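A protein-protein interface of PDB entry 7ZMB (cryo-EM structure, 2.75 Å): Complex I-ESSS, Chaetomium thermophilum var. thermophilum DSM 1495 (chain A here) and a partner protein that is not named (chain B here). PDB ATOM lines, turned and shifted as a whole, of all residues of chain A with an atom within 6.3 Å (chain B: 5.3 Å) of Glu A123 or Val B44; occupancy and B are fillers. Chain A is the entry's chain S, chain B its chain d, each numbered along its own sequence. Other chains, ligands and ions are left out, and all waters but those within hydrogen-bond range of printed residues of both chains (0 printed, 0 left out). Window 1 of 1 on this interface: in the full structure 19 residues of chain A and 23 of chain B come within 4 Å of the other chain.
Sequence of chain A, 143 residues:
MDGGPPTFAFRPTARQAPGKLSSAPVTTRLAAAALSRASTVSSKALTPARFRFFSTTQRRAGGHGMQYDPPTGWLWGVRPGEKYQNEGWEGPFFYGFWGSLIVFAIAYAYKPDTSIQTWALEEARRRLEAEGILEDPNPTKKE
Trp A119 touches Phe B9 (O to CE2, 3.2 Å).
Met B47 touches Ala A120.
Leu A121 touches Met B47 (CD2 to CE, 3.4 Å).
CZ of Phe B9 touches OE2 of Glu A123 (3.2 Å).
Ala A124 touches Val B44 (CB to O, 3.7 Å).
Ala A124 touches Met B48.
NH1 of Arg A126 touches CE2 of Phe B9 (3.2 Å).
Arg A127 touches Gln B45 (NE to OE1, 3.8 Å).
Arg A127 touches Met B48 (CD to SD, 3.7 Å).
CE of Met B48 touches CD1 of Leu A128, 3.5 Å away.
NH2 of Arg A126 lies within salt-bridge range of OE2 of Glu A122 (3.7 Å).
OE1 of Gln B45 lies close to SD of Met B48 (3.2 Å).
The side-chain amide oxygen (OE1) of Gln B45 sits close to the side-chain carboxylate (OE2) of Glu B41.
The guanidinium group (NE) of Arg A126 lies within salt-bridge range of the side-chain carboxylate (OE2) of Glu A123 (3.7 Å).
The side-chain carboxylate of Glu A123 is in salt-bridge range of the guanidinium group of Arg A127 (3.4 Å).
The side-chain carboxylate (OE1) of Glu B41 lies within salt-bridge range of the guanidinium group (NH2) of Arg A127 (3.1 Å).
Of the 12 printed residues of chain B, 8 touch a printed residue of chain A.
Along chain B the printed residues that touch a printed residue of chain A span positions 9 to 48.
Among the printed residues, 18 pairs touch across the chains.
Of chain B, only Phe B9 and Val B44 come within 4 Å of Glu A123.
Printed residues of chain B within 4 Å of Arg A126: Phe B9.
Printed residues of chain A within 4 Å of Lys B13: Trp A119.
Ile B39 touches none of the printed residues of chain A.
Printed residues of chain A within 4 Å of Glu B41: Arg A127 (3.1 Å).
Gln B42 touches none of the printed residues of chain A.
Val B44 touches just these residues of chain A: Trp A119 (3.5 Å), Ala A120 (3.8 Å), Glu A123 (3.6 Å), Ala A124 (3.7 Å) and Arg A127 (3.6 Å).
Of the printed residues of chain A, Met B48 touches Ala A124 (3.5 Å), Arg A127 (3.7 Å) and Leu A128 (3.5 Å).
The nearest printed residue of chain B that does not touch Leu A121 is Val B44 (5.7 Å).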
ATOM      1  N   THR A 118      28.172  16.848 -23.654  1.00  0.00           N
ATOM      2  CA  THR A 118      29.418  16.125 -23.419  1.00  0.00           C
ATOM      3  C   THR A 118      30.053  16.520 -22.091  1.00  0.00           C
ATOM      4  O   THR A 118      30.513  15.660 -21.334  1.00  0.00           O
ATOM      5  CB  THR A 118      30.377  16.393 -24.575  1.00  0.00           C
ATOM      6  OG1 THR A 118      29.947  15.664 -25.728  1.00  0.00           O
ATOM      7  CG2 THR A 118      31.790  15.982 -24.212  1.00  0.00           C
ATOM      8  N   TRP A 119      30.090  17.821 -21.794  1.00  0.00           N
ATOM      9  CA  TRP A 119      30.664  18.280 -20.534  1.00  0.00           C
ATOM     10  C   TRP A 119      29.829  17.812 -19.354  1.00  0.00           C
ATOM     11  O   TRP A 119      30.369  17.437 -18.309  1.00  0.00           O
ATOM     12  CB  TRP A 119      30.784  19.806 -20.531  1.00  0.00           C
ATOM     13  CG  TRP A 119      31.380  20.383 -19.279  1.00  0.00           C
ATOM     14  CD1 TRP A 119      32.689  20.668 -19.063  1.00  0.00           C
ATOM     15  CD2 TRP A 119      30.690  20.748 -18.079  1.00  0.00           C
ATOM     16  NE1 TRP A 119      32.865  21.182 -17.809  1.00  0.00           N
ATOM     17  CE2 TRP A 119      31.651  21.243 -17.183  1.00  0.00           C
ATOM     18  CE3 TRP A 119      29.357  20.702 -17.674  1.00  0.00           C
ATOM     19  CZ2 TRP A 119      31.321  21.686 -15.907  1.00  0.00           C
ATOM     20  CZ3 TRP A 119      29.033  21.144 -16.417  1.00  0.00           C
ATOM     21  CH2 TRP A 119      30.009  21.629 -15.546  1.00  0.00           C
ATOM     22  N   ALA A 120      28.510  17.846 -19.500  1.00  0.00           N
ATOM     23  CA  ALA A 120      27.631  17.485 -18.400  1.00  0.00           C
ATOM     24  C   ALA A 120      27.556  15.978 -18.199  1.00  0.00           C
ATOM     25  O   ALA A 120      27.346  15.530 -17.068  1.00  0.00           O
ATOM     26  CB  ALA A 120      26.245  18.081 -18.629  1.00  0.00           C
ATOM     27  N   LEU A 121      27.725  15.180 -19.260  1.00  0.00           N
ATOM     28  CA  LEU A 121      27.873  13.738 -19.072  1.00  0.00           C
ATOM     29  C   LEU A 121      28.951  13.426 -18.053  1.00  0.00           C
ATOM     30  O   LEU A 121      28.736  12.637 -17.128  1.00  0.00           O
ATOM     31  CB  LEU A 121      28.201  13.021 -20.383  1.00  0.00           C
ATOM     32  CG  LEU A 121      27.198  12.476 -21.406  1.00  0.00           C
ATOM     33  CD1 LEU A 121      26.376  11.363 -20.771  1.00  0.00           C
ATOM     34  CD2 LEU A 121      26.302  13.485 -22.020  1.00  0.00           C
ATOM     35  N   GLU A 122      30.124  14.038 -18.210  1.00  0.00           N
ATOM     36  CA  GLU A 122      31.253  13.687 -17.361  1.00  0.00           C
ATOM     37  C   GLU A 122      30.963  14.004 -15.904  1.00  0.00           C
ATOM     38  O   GLU A 122      31.194  13.172 -15.020  1.00  0.00           O
ATOM     39  CB  GLU A 122      32.514  14.405 -17.841  1.00  0.00           C
ATOM     40  CG  GLU A 122      33.775  13.570 -17.682  1.00  0.00           C
ATOM     41  CD  GLU A 122      35.003  14.251 -18.246  1.00  0.00           C
ATOM     42  OE1 GLU A 122      34.871  15.376 -18.769  1.00  0.00           O
ATOM     43  OE2 GLU A 122      36.101  13.662 -18.162  1.00  0.00           O
ATOM     44  N   GLU A 123      30.445  15.200 -15.631  1.00  0.00           N
ATOM     45  CA  GLU A 123      30.127  15.554 -14.253  1.00  0.00           C
ATOM     46  C   GLU A 123      29.056  14.638 -13.692  1.00  0.00           C
ATOM     47  O   GLU A 123      29.221  14.057 -12.614  1.00  0.00           O
ATOM     48  CB  GLU A 123      29.673  17.005 -14.169  1.00  0.00           C
ATOM     49  CG  GLU A 123      29.322  17.454 -12.760  1.00  0.00           C
ATOM     50  CD  GLU A 123      30.505  17.378 -11.812  1.00  0.00           C
ATOM     51  OE1 GLU A 123      30.286  17.119 -10.610  1.00  0.00           O
ATOM     52  OE2 GLU A 123      31.651  17.573 -12.270  1.00  0.00           O
ATOM     53  N   ALA A 124      27.952  14.485 -14.421  1.00  0.00           N
ATOM     54  CA  ALA A 124      26.884  13.609 -13.966  1.00  0.00           C
ATOM     55  C   ALA A 124      27.372  12.173 -13.817  1.00  0.00           C
ATOM     56  O   ALA A 124      26.887  11.442 -12.950  1.00  0.00           O
ATOM     57  CB  ALA A 124      25.707  13.690 -14.931  1.00  0.00           C
ATOM     58  N   ARG A 125      28.327  11.751 -14.653  1.00  0.00           N
ATOM     59  CA  ARG A 125      28.925  10.433 -14.485  1.00  0.00           C
ATOM     60  C   ARG A 125      29.704  10.354 -13.179  1.00  0.00           C
ATOM     61  O   ARG A 125      29.630   9.347 -12.466  1.00  0.00           O
ATOM     62  CB  ARG A 125      29.826  10.107 -15.675  1.00  0.00           C
ATOM     63  CG  ARG A 125      30.721   8.897 -15.479  1.00  0.00           C
ATOM     64  CD  ARG A 125      29.907   7.622 -15.368  1.00  0.00           C
ATOM     65  NE  ARG A 125      29.301   7.253 -16.643  1.00  0.00           N
ATOM     66  CZ  ARG A 125      29.945   6.632 -17.625  1.00  0.00           C
ATOM     67  NH1 ARG A 125      29.312   6.335 -18.751  1.00  0.00           N
ATOM     68  NH2 ARG A 125      31.222   6.307 -17.481  1.00  0.00           N
ATOM     69  N   ARG A 126      30.451  11.407 -12.849  1.00  0.00           N
ATOM     70  CA  ARG A 126      31.059  11.496 -11.527  1.00  0.00           C
ATOM     71  C   ARG A 126      30.003  11.679 -10.448  1.00  0.00           C
ATOM     72  O   ARG A 126      30.159  11.176  -9.331  1.00  0.00           O
ATOM     73  CB  ARG A 126      32.058  12.646 -11.477  1.00  0.00           C
ATOM     74  CG  ARG A 126      33.447  12.312 -11.960  1.00  0.00           C
ATOM     75  CD  ARG A 126      34.296  13.563 -11.953  1.00  0.00           C
ATOM     76  NE  ARG A 126      33.783  14.552 -12.891  1.00  0.00           N
ATOM     77  CZ  ARG A 126      34.150  14.628 -14.163  1.00  0.00           C
ATOM     78  NH1 ARG A 126      33.631  15.557 -14.950  1.00  0.00           N
ATOM     79  NH2 ARG A 126      35.044  13.777 -14.646  1.00  0.00           N
ATOM     80  N   ARG A 127      28.931  12.414 -10.757  1.00  0.00           N
ATOM     81  CA  ARG A 127      27.920  12.707  -9.745  1.00  0.00           C
ATOM     82  C   ARG A 127      27.245  11.437  -9.249  1.00  0.00           C
ATOM     83  O   ARG A 127      27.028  11.272  -8.044  1.00  0.00           O
ATOM     84  CB  ARG A 127      26.883  13.683 -10.298  1.00  0.00           C
ATOM     85  CG  ARG A 127      27.311  15.134 -10.286  1.00  0.00           C
ATOM     86  CD  ARG A 127      26.197  16.027  -9.747  1.00  0.00           C
ATOM     87  NE  ARG A 127      26.511  17.449  -9.863  1.00  0.00           N
ATOM     88  CZ  ARG A 127      27.386  18.084  -9.094  1.00  0.00           C
ATOM     89  NH1 ARG A 127      28.038  17.427  -8.145  1.00  0.00           N
ATOM     90  NH2 ARG A 127      27.609  19.378  -9.270  1.00  0.00           N
ATOM     91  N   LEU A 128      26.905  10.526 -10.160  1.00  0.00           N
ATOM     92  CA  LEU A 128      26.307   9.265  -9.739  1.00  0.00           C
ATOM     93  C   LEU A 128      27.319   8.327  -9.100  1.00  0.00           C
ATOM     94  O   LEU A 128      26.926   7.447  -8.328  1.00  0.00           O
ATOM     95  CB  LEU A 128      25.635   8.560 -10.918  1.00  0.00           C
ATOM     96  CG  LEU A 128      24.188   8.932 -11.251  1.00  0.00           C
ATOM     97  CD1 LEU A 128      24.092  10.272 -11.936  1.00  0.00           C
ATOM     98  CD2 LEU A 128      23.551   7.844 -12.097  1.00  0.00           C
ATOM     99  N   PHE B   9      37.402  18.819 -19.466  1.00  0.00           N
ATOM    100  CA  PHE B   9      36.683  19.257 -18.273  1.00  0.00           C
ATOM    101  C   PHE B   9      37.622  20.029 -17.343  1.00  0.00           C
ATOM    102  O   PHE B   9      37.742  19.750 -16.155  1.00  0.00           O
ATOM    103  CB  PHE B   9      36.081  18.038 -17.585  1.00  0.00           C
ATOM    104  CG  PHE B   9      34.948  18.340 -16.640  1.00  0.00           C
ATOM    105  CD1 PHE B   9      35.178  18.865 -15.383  1.00  0.00           C
ATOM    106  CD2 PHE B   9      33.649  18.053 -17.001  1.00  0.00           C
ATOM    107  CE1 PHE B   9      34.147  19.122 -14.534  1.00  0.00           C
ATOM    108  CE2 PHE B   9      32.610  18.306 -16.142  1.00  0.00           C
ATOM    109  CZ  PHE B   9      32.862  18.838 -14.912  1.00  0.00           C
ATOM    110  N   LYS B  13      34.835  23.933 -16.799  1.00  0.00           N
ATOM    111  CA  LYS B  13      34.409  23.829 -15.417  1.00  0.00           C
ATOM    112  C   LYS B  13      34.210  25.224 -14.844  1.00  0.00           C
ATOM    113  O   LYS B  13      35.110  26.061 -14.949  1.00  0.00           O
ATOM    114  CB  LYS B  13      35.429  23.069 -14.589  1.00  0.00           C
ATOM    115  CG  LYS B  13      35.011  22.866 -13.144  1.00  0.00           C
ATOM    116  CD  LYS B  13      35.999  21.988 -12.399  1.00  0.00           C
ATOM    117  CE  LYS B  13      35.286  21.076 -11.417  1.00  0.00           C
ATOM    118  NZ  LYS B  13      34.468  21.847 -10.443  1.00  0.00           N
ATOM    119  N   ILE B  39      23.825  27.762 -15.490  1.00  0.00           N
ATOM    120  CA  ILE B  39      23.476  26.924 -16.629  1.00  0.00           C
ATOM    121  C   ILE B  39      24.153  25.563 -16.535  1.00  0.00           C
ATOM    122  O   ILE B  39      23.585  24.551 -16.965  1.00  0.00           O
ATOM    123  CB  ILE B  39      23.825  27.648 -17.943  1.00  0.00           C
ATOM    124  CG1 ILE B  39      22.934  28.878 -18.128  1.00  0.00           C
ATOM    125  CG2 ILE B  39      23.655  26.733 -19.127  1.00  0.00           C
ATOM    126  CD1 ILE B  39      21.488  28.626 -17.878  1.00  0.00           C
ATOM    127  N   ARG B  40      25.393  25.527 -16.049  1.00  0.00           N
ATOM    128  CA  ARG B  40      26.182  24.264 -15.983  1.00  0.00           C
ATOM    129  C   ARG B  40      25.511  23.250 -15.053  1.00  0.00           C
ATOM    130  O   ARG B  40      25.530  22.058 -15.386  1.00  0.00           O
ATOM    131  CB  ARG B  40      27.602  24.552 -15.495  1.00  0.00           C
ATOM    132  CG  ARG B  40      28.445  25.359 -16.469  1.00  0.00           C
ATOM    133  CD  ARG B  40      28.963  24.546 -17.633  1.00  0.00           C
ATOM    134  NE  ARG B  40      29.494  25.426 -18.655  1.00  0.00           N
ATOM    135  CZ  ARG B  40      30.158  25.021 -19.725  1.00  0.00           C
ATOM    136  NH1 ARG B  40      30.387  23.734 -19.914  1.00  0.00           N
ATOM    137  NH2 ARG B  40      30.593  25.906 -20.600  1.00  0.00           N
ATOM    138  N   GLU B  41      24.930  23.707 -13.942  1.00  0.00           N
ATOM    139  CA  GLU B  41      24.350  22.789 -12.926  1.00  0.00           C
ATOM    140  C   GLU B  41      23.028  22.210 -13.423  1.00  0.00           C
ATOM    141  O   GLU B  41      22.834  20.992 -13.289  1.00  0.00           O
ATOM    142  CB  GLU B  41      24.107  23.548 -11.626  1.00  0.00           C
ATOM    143  CG  GLU B  41      23.602  22.671 -10.495  1.00  0.00           C
ATOM    144  CD  GLU B  41      24.557  21.575 -10.053  1.00  0.00           C
ATOM    145  OE1 GLU B  41      25.781  21.807 -10.089  1.00  0.00           O
ATOM    146  OE2 GLU B  41      24.072  20.488  -9.682  1.00  0.00           O
ATOM    147  N   GLN B  42      22.160  23.061 -13.963  1.00  0.00           N
ATOM    148  CA  GLN B  42      20.838  22.621 -14.458  1.00  0.00           C
ATOM    149  C   GLN B  42      21.070  21.575 -15.540  1.00  0.00           C
ATOM    150  O   GLN B  42      20.299  20.607 -15.588  1.00  0.00           O
ATOM    151  CB  GLN B  42      20.061  23.808 -15.026  1.00  0.00           C
ATOM    152  CG  GLN B  42      19.626  24.832 -13.993  1.00  0.00           C
ATOM    153  CD  GLN B  42      18.883  25.949 -14.678  1.00  0.00           C
ATOM    154  OE1 GLN B  42      18.961  26.111 -15.892  1.00  0.00           O
ATOM    155  NE2 GLN B  42      18.150  26.730 -13.901  1.00  0.00           N
ATOM    156  N   TRP B  43      22.127  21.748 -16.333  1.00  0.00           N
ATOM    157  CA  TRP B  43      22.367  20.809 -17.453  1.00  0.00           C
ATOM    158  C   TRP B  43      22.931  19.505 -16.882  1.00  0.00           C
ATOM    159  O   TRP B  43      22.459  18.453 -17.321  1.00  0.00           O
ATOM    160  CB  TRP B  43      23.299  21.433 -18.502  1.00  0.00           C
ATOM    161  CG  TRP B  43      22.581  22.016 -19.680  1.00  0.00           C
ATOM    162  CD1 TRP B  43      22.412  23.336 -19.976  1.00  0.00           C
ATOM    163  CD2 TRP B  43      21.921  21.284 -20.728  1.00  0.00           C
ATOM    164  NE1 TRP B  43      21.698  23.477 -21.134  1.00  0.00           N
ATOM    165  CE2 TRP B  43      21.382  22.236 -21.619  1.00  0.00           C
ATOM    166  CE3 TRP B  43      21.733  19.925 -20.999  1.00  0.00           C
ATOM    167  CZ2 TRP B  43      20.665  21.869 -22.755  1.00  0.00           C
ATOM    168  CZ3 TRP B  43      21.028  19.564 -22.124  1.00  0.00           C
ATOM    169  CH2 TRP B  43      20.503  20.524 -22.989  1.00  0.00           C
ATOM    170  N   VAL B  44      23.848  19.560 -15.912  1.00  0.00           N
ATOM    171  CA  VAL B  44      24.337  18.330 -15.296  1.00  0.00           C
ATOM    172  C   VAL B  44      23.190  17.569 -14.652  1.00  0.00           C
ATOM    173  O   VAL B  44      23.085  16.345 -14.783  1.00  0.00           O
ATOM    174  CB  VAL B  44      25.450  18.633 -14.276  1.00  0.00           C
ATOM    175  CG1 VAL B  44      25.612  17.470 -13.308  1.00  0.00           C
ATOM    176  CG2 VAL B  44      26.751  18.900 -14.994  1.00  0.00           C
ATOM    177  N   GLN B  45      22.303  18.286 -13.964  1.00  0.00           N
ATOM    178  CA  GLN B  45      21.183  17.639 -13.295  1.00  0.00           C
ATOM    179  C   GLN B  45      20.287  16.917 -14.285  1.00  0.00           C
ATOM    180  O   GLN B  45      19.826  15.803 -14.013  1.00  0.00           O
ATOM    181  CB  GLN B  45      20.386  18.670 -12.501  1.00  0.00           C
ATOM    182  CG  GLN B  45      20.993  19.000 -11.166  1.00  0.00           C
ATOM    183  CD  GLN B  45      21.493  17.766 -10.449  1.00  0.00           C
ATOM    184  OE1 GLN B  45      22.697  17.535 -10.353  1.00  0.00           O
ATOM    185  NE2 GLN B  45      20.567  16.963  -9.944  1.00  0.00           N
ATOM    186  N   VAL B  46      20.022  17.534 -15.439  1.00  0.00           N
ATOM    187  CA  VAL B  46      19.215  16.886 -16.467  1.00  0.00           C
ATOM    188  C   VAL B  46      19.921  15.647 -16.995  1.00  0.00           C
ATOM    189  O   VAL B  46      19.289  14.612 -17.236  1.00  0.00           O
ATOM    190  CB  VAL B  46      18.886  17.874 -17.601  1.00  0.00           C
ATOM    191  CG1 VAL B  46      18.139  17.174 -18.722  1.00  0.00           C
ATOM    192  CG2 VAL B  46      18.066  19.025 -17.080  1.00  0.00           C
ATOM    193  N   MET B  47      21.238  15.728 -17.186  1.00  0.00           N
ATOM    194  CA  MET B  47      21.954  14.582 -17.729  1.00  0.00           C
ATOM    195  C   MET B  47      22.092  13.446 -16.732  1.00  0.00           C
ATOM    196  O   MET B  47      22.391  12.323 -17.145  1.00  0.00           O
ATOM    197  CB  MET B  47      23.331  14.987 -18.236  1.00  0.00           C
ATOM    198  CG  MET B  47      23.305  16.192 -19.116  1.00  0.00           C
ATOM    199  SD  MET B  47      22.301  16.031 -20.590  1.00  0.00           S
ATOM    200  CE  MET B  47      23.265  14.857 -21.504  1.00  0.00           C
ATOM    201  N   MET B  48      21.884  13.696 -15.440  1.00  0.00           N
ATOM    202  CA  MET B  48      21.778  12.582 -14.506  1.00  0.00           C
ATOM    203  C   MET B  48      20.570  11.722 -14.830  1.00  0.00           C
ATOM    204  O   MET B  48      20.643  10.490 -14.765  1.00  0.00           O
ATOM    205  CB  MET B  48      21.737  13.093 -13.068  1.00  0.00           C
ATOM    206  CG  MET B  48      23.044  13.735 -12.644  1.00  0.00           C
ATOM    207  SD  MET B  48      23.102  14.452 -11.005  1.00  0.00           S
ATOM    208  CE  MET B  48      23.068  13.007  -9.959  1.00  0.00           C
